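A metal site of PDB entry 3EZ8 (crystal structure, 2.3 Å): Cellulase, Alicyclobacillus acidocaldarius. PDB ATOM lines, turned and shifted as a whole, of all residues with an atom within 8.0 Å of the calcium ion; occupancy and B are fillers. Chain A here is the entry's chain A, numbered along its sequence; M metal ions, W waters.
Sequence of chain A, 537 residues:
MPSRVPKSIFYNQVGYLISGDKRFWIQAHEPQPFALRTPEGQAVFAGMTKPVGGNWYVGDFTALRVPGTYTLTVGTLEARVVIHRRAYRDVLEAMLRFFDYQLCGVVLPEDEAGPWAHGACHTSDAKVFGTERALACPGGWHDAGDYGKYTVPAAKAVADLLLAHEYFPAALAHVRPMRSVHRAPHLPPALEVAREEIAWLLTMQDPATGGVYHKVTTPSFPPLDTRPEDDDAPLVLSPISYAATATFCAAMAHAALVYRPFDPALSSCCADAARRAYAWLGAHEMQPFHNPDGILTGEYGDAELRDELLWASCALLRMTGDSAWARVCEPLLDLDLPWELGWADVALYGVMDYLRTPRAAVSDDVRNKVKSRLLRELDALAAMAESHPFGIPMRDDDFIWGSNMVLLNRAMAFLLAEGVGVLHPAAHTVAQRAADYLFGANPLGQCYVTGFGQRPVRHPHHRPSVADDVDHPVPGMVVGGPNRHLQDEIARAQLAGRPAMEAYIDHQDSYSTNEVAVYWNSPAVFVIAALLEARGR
The calcium ion is bound by the backbone carbonyl oxygen (O) of Ala 344 (2.4 Å), the side-chain carboxylate (OD2) of Asp 302 (2.4 Å), the side-chain carboxylate (OE2) of Glu 308 (2.4 Å), the side-chain carboxylate (OE1) of Glu 308 (2.5 Å), the side-chain carboxylate (OD1) of Asp 307 (2.5 Å), the side-chain carboxylate (OD2) of Asp 307 (2.5 Å), water W1 (2.6 Å) and the backbone carbonyl oxygen (O) of Glu 304 (2.6 Å).
Water W1 lies within hydrogen-bond range of OD1 of Asp 345 (2.4 Å) and OD1 of Asp 302 (2.8 Å).
The side-chain carboxylate of Asp 307 sits close to the backbone NH of Val 346. NH2 of Arg 306 is in salt-bridge range of OE2 of Glu 304.
Within 4 Å of the calcium ion: Asp 302, Glu 304, Asp 307, Glu 308 and Ala 344. The nearest printed residue that does not touch the calcium ion is Asp 345 (4.2 Å).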
ATOM      1  N   VAL A 152     -34.424 -37.084  22.656  1.00  0.00           N
ATOM      2  CA  VAL A 152     -33.195 -36.422  23.120  1.00  0.00           C
ATOM      3  C   VAL A 152     -32.311 -37.321  24.010  1.00  0.00           C
ATOM      4  O   VAL A 152     -31.125 -37.496  23.704  1.00  0.00           O
ATOM      5  CB  VAL A 152     -33.496 -35.051  23.814  1.00  0.00           C
ATOM      6  CG1 VAL A 152     -32.207 -34.408  24.337  1.00  0.00           C
ATOM      7  CG2 VAL A 152     -34.193 -34.097  22.846  1.00  0.00           C
ATOM      8  N   ALA A 243     -34.314 -29.643  19.324  1.00  0.00           N
ATOM      9  CA  ALA A 243     -33.461 -30.491  20.158  1.00  0.00           C
ATOM     10  C   ALA A 243     -33.498 -31.944  19.706  1.00  0.00           C
ATOM     11  O   ALA A 243     -32.457 -32.574  19.564  1.00  0.00           O
ATOM     12  CB  ALA A 243     -33.878 -30.381  21.616  1.00  0.00           C
ATOM     13  N   GLY A 301     -36.669 -30.678  28.396  1.00  0.00           N
ATOM     14  CA  GLY A 301     -36.498 -29.332  27.873  1.00  0.00           C
ATOM     15  C   GLY A 301     -35.055 -28.862  28.007  1.00  0.00           C
ATOM     16  O   GLY A 301     -34.255 -29.459  28.733  1.00  0.00           O
ATOM     17  N   ASP A 302     -34.748 -27.777  27.305  1.00  0.00           N
ATOM     18  CA  ASP A 302     -33.389 -27.255  27.193  1.00  0.00           C
ATOM     19  C   ASP A 302     -33.450 -25.923  26.454  1.00  0.00           C
ATOM     20  O   ASP A 302     -34.126 -25.816  25.432  1.00  0.00           O
ATOM     21  CB  ASP A 302     -32.506 -28.236  26.428  1.00  0.00           C
ATOM     22  CG  ASP A 302     -31.036 -27.890  26.495  1.00  0.00           C
ATOM     23  OD1 ASP A 302     -30.617 -27.153  27.410  1.00  0.00           O
ATOM     24  OD2 ASP A 302     -30.281 -28.373  25.611  1.00  0.00           O
ATOM     25  N   ALA A 303     -32.744 -24.920  26.970  1.00  0.00           N
ATOM     26  CA  ALA A 303     -32.799 -23.561  26.414  1.00  0.00           C
ATOM     27  C   ALA A 303     -31.689 -23.269  25.411  1.00  0.00           C
ATOM     28  O   ALA A 303     -31.827 -22.411  24.549  1.00  0.00           O
ATOM     29  CB  ALA A 303     -32.798 -22.536  27.538  1.00  0.00           C
ATOM     30  N   GLU A 304     -30.576 -23.986  25.549  1.00  0.00           N
ATOM     31  CA  GLU A 304     -29.426 -23.816  24.677  1.00  0.00           C
ATOM     32  C   GLU A 304     -29.391 -24.931  23.629  1.00  0.00           C
ATOM     33  O   GLU A 304     -29.358 -26.115  23.981  1.00  0.00           O
ATOM     34  CB  GLU A 304     -28.140 -23.817  25.512  1.00  0.00           C
ATOM     35  CG  GLU A 304     -26.851 -23.748  24.718  1.00  0.00           C
ATOM     36  CD  GLU A 304     -26.642 -22.402  24.033  1.00  0.00           C
ATOM     37  OE1 GLU A 304     -27.291 -21.406  24.410  1.00  0.00           O
ATOM     38  OE2 GLU A 304     -25.797 -22.354  23.118  1.00  0.00           O
ATOM     39  N   LEU A 305     -29.417 -24.549  22.362  1.00  0.00           N
ATOM     40  CA  LEU A 305     -29.461 -25.538  21.285  1.00  0.00           C
ATOM     41  C   LEU A 305     -28.271 -25.459  20.322  1.00  0.00           C
ATOM     42  O   LEU A 305     -28.244 -26.140  19.298  1.00  0.00           O
ATOM     43  CB  LEU A 305     -30.808 -25.470  20.527  1.00  0.00           C
ATOM     44  CG  LEU A 305     -32.073 -25.695  21.373  1.00  0.00           C
ATOM     45  CD1 LEU A 305     -33.325 -25.423  20.567  1.00  0.00           C
ATOM     46  CD2 LEU A 305     -32.114 -27.097  21.976  1.00  0.00           C
ATOM     47  N   ARG A 306     -27.289 -24.636  20.677  1.00  0.00           N
ATOM     48  CA  ARG A 306     -26.065 -24.493  19.881  1.00  0.00           C
ATOM     49  C   ARG A 306     -25.130 -25.688  20.023  1.00  0.00           C
ATOM     50  O   ARG A 306     -24.414 -26.018  19.068  1.00  0.00           O
ATOM     51  CB  ARG A 306     -25.319 -23.194  20.233  1.00  0.00           C
ATOM     52  CG  ARG A 306     -25.945 -21.933  19.651  1.00  0.00           C
ATOM     53  CD  ARG A 306     -25.249 -20.682  20.166  1.00  0.00           C
ATOM     54  NE  ARG A 306     -25.353 -20.538  21.613  1.00  0.00           N
ATOM     55  CZ  ARG A 306     -24.736 -19.613  22.344  1.00  0.00           C
ATOM     56  NH1 ARG A 306     -23.956 -18.717  21.760  1.00  0.00           N
ATOM     57  NH2 ARG A 306     -24.900 -19.585  23.658  1.00  0.00           N
ATOM     58  N   ASP A 307     -25.122 -26.332  21.188  1.00  0.00           N
ATOM     59  CA  ASP A 307     -24.324 -27.540  21.391  1.00  0.00           C
ATOM     60  C   ASP A 307     -24.925 -28.750  20.683  1.00  0.00           C
ATOM     61  O   ASP A 307     -24.220 -29.713  20.377  1.00  0.00           O
ATOM     62  CB  ASP A 307     -24.106 -27.821  22.882  1.00  0.00           C
ATOM     63  CG  ASP A 307     -25.399 -27.928  23.656  1.00  0.00           C
ATOM     64  OD1 ASP A 307     -26.134 -26.923  23.737  1.00  0.00           O
ATOM     65  OD2 ASP A 307     -25.678 -29.012  24.198  1.00  0.00           O
ATOM     66  N   GLU A 308     -26.229 -28.694  20.416  1.00  0.00           N
ATOM     67  CA  GLU A 308     -26.924 -29.698  19.616  1.00  0.00           C
ATOM     68  C   GLU A 308     -26.571 -29.550  18.138  1.00  0.00           C
ATOM     69  O   GLU A 308     -26.307 -30.539  17.449  1.00  0.00           O
ATOM     70  CB  GLU A 308     -28.434 -29.603  19.798  1.00  0.00           C
ATOM     71  CG  GLU A 308     -28.973 -30.280  21.063  1.00  0.00           C
ATOM     72  CD  GLU A 308     -28.733 -29.485  22.343  1.00  0.00           C
ATOM     73  OE1 GLU A 308     -28.281 -28.331  22.260  1.00  0.00           O
ATOM     74  OE2 GLU A 308     -29.002 -30.030  23.431  1.00  0.00           O
ATOM     75  N   LEU A 309     -26.573 -28.298  17.661  1.00  0.00           N
ATOM     76  CA  LEU A 309     -26.164 -27.985  16.287  1.00  0.00           C
ATOM     77  C   LEU A 309     -24.691 -28.319  16.074  1.00  0.00           C
ATOM     78  O   LEU A 309     -24.308 -28.813  15.007  1.00  0.00           O
ATOM     79  CB  LEU A 309     -26.425 -26.496  15.982  1.00  0.00           C
ATOM     80  CG  LEU A 309     -26.108 -25.949  14.586  1.00  0.00           C
ATOM     81  CD1 LEU A 309     -26.975 -26.602  13.504  1.00  0.00           C
ATOM     82  CD2 LEU A 309     -26.282 -24.444  14.553  1.00  0.00           C
ATOM     83  N   LEU A 337     -19.440 -22.946  25.330  1.00  0.00           N
ATOM     84  CA  LEU A 337     -20.345 -24.019  25.704  1.00  0.00           C
ATOM     85  C   LEU A 337     -19.648 -25.017  26.630  1.00  0.00           C
ATOM     86  O   LEU A 337     -18.464 -25.298  26.435  1.00  0.00           O
ATOM     87  CB  LEU A 337     -20.849 -24.761  24.459  1.00  0.00           C
ATOM     88  CG  LEU A 337     -21.787 -24.042  23.492  1.00  0.00           C
ATOM     89  CD1 LEU A 337     -21.773 -24.729  22.135  1.00  0.00           C
ATOM     90  CD2 LEU A 337     -23.192 -23.989  24.053  1.00  0.00           C
ATOM     91  N   PRO A 338     -20.372 -25.536  27.641  1.00  0.00           N
ATOM     92  CA  PRO A 338     -19.804 -26.628  28.430  1.00  0.00           C
ATOM     93  C   PRO A 338     -19.595 -27.857  27.535  1.00  0.00           C
ATOM     94  O   PRO A 338     -20.486 -28.211  26.759  1.00  0.00           O
ATOM     95  CB  PRO A 338     -20.876 -26.899  29.484  1.00  0.00           C
ATOM     96  CG  PRO A 338     -22.129 -26.296  28.946  1.00  0.00           C
ATOM     97  CD  PRO A 338     -21.684 -25.116  28.141  1.00  0.00           C
ATOM     98  N   GLY A 342     -24.116 -34.830  27.719  1.00  0.00           N
ATOM     99  CA  GLY A 342     -25.571 -34.925  27.752  1.00  0.00           C
ATOM    100  C   GLY A 342     -26.206 -35.197  29.110  1.00  0.00           C
ATOM    101  O   GLY A 342     -25.513 -35.203  30.133  1.00  0.00           O
ATOM    102  N   TRP A 343     -27.524 -35.407  29.135  1.00  0.00           N
ATOM    103  CA  TRP A 343     -28.351 -35.428  27.919  1.00  0.00           C
ATOM    104  C   TRP A 343     -28.638 -34.049  27.342  1.00  0.00           C
ATOM    105  O   TRP A 343     -28.900 -33.907  26.148  1.00  0.00           O
ATOM    106  CB  TRP A 343     -29.679 -36.160  28.183  1.00  0.00           C
ATOM    107  CG  TRP A 343     -30.491 -35.564  29.291  1.00  0.00           C
ATOM    108  CD1 TRP A 343     -30.491 -35.957  30.601  1.00  0.00           C
ATOM    109  CD2 TRP A 343     -31.418 -34.467  29.206  1.00  0.00           C
ATOM    110  NE1 TRP A 343     -31.361 -35.174  31.327  1.00  0.00           N
ATOM    111  CE2 TRP A 343     -31.940 -34.251  30.498  1.00  0.00           C
ATOM    112  CE3 TRP A 343     -31.853 -33.651  28.152  1.00  0.00           C
ATOM    113  CZ2 TRP A 343     -32.876 -33.254  30.776  1.00  0.00           C
ATOM    114  CZ3 TRP A 343     -32.789 -32.654  28.429  1.00  0.00           C
ATOM    115  CH2 TRP A 343     -33.287 -32.467  29.721  1.00  0.00           C
ATOM    116  N   ALA A 344     -28.580 -33.020  28.197  1.00  0.00           N
ATOM    117  CA  ALA A 344     -28.935 -31.656  27.805  1.00  0.00           C
ATOM    118  C   ALA A 344     -27.787 -30.881  27.164  1.00  0.00           C
ATOM    119  O   ALA A 344     -28.000 -30.093  26.234  1.00  0.00           O
ATOM    120  CB  ALA A 344     -29.481 -30.895  29.015  1.00  0.00           C
ATOM    121  N   ASP A 345     -26.581 -31.131  27.597  1.00  0.00           N
ATOM    122  CA  ASP A 345     -25.414 -30.441  27.141  1.00  0.00           C
ATOM    123  C   ASP A 345     -24.464 -31.407  26.462  1.00  0.00           C
ATOM    124  O   ASP A 345     -23.723 -32.035  27.107  1.00  0.00           O
ATOM    125  CB  ASP A 345     -24.717 -29.756  28.321  1.00  0.00           C
ATOM    126  CG  ASP A 345     -25.599 -28.765  29.036  1.00  0.00           C
ATOM    127  OD1 ASP A 345     -25.996 -27.808  28.458  1.00  0.00           O
ATOM    128  OD2 ASP A 345     -25.966 -29.018  30.148  1.00  0.00           O
ATOM    129  N   VAL A 346     -24.483 -31.442  25.144  1.00  0.00           N
ATOM    130  CA  VAL A 346     -23.909 -32.539  24.359  1.00  0.00           C
ATOM    131  C   VAL A 346     -22.676 -32.155  23.515  1.00  0.00           C
ATOM    132  O   VAL A 346     -22.302 -32.887  22.590  1.00  0.00           O
ATOM    133  CB  VAL A 346     -24.973 -33.181  23.425  1.00  0.00           C
ATOM    134  CG1 VAL A 346     -26.007 -33.949  24.237  1.00  0.00           C
ATOM    135  CG2 VAL A 346     -25.646 -32.124  22.540  1.00  0.00           C
ATOM    136  N   ALA A 347     -22.050 -31.032  23.865  1.00  0.00           N
ATOM    137  CA  ALA A 347     -20.939 -30.472  23.073  1.00  0.00           C
ATOM    138  C   ALA A 347     -19.737 -31.403  22.915  1.00  0.00           C
ATOM    139  O   ALA A 347     -19.089 -31.386  21.867  1.00  0.00           O
ATOM    140  CB  ALA A 347     -20.510 -29.133  23.663  1.00  0.00           C
HETATM  141 CA    CA M   1     -28.037 -28.243  24.762  1.00  0.00          CA
HETATM  142  O   HOH W   1     -27.858 -27.095  27.055  1.00  0.00           O
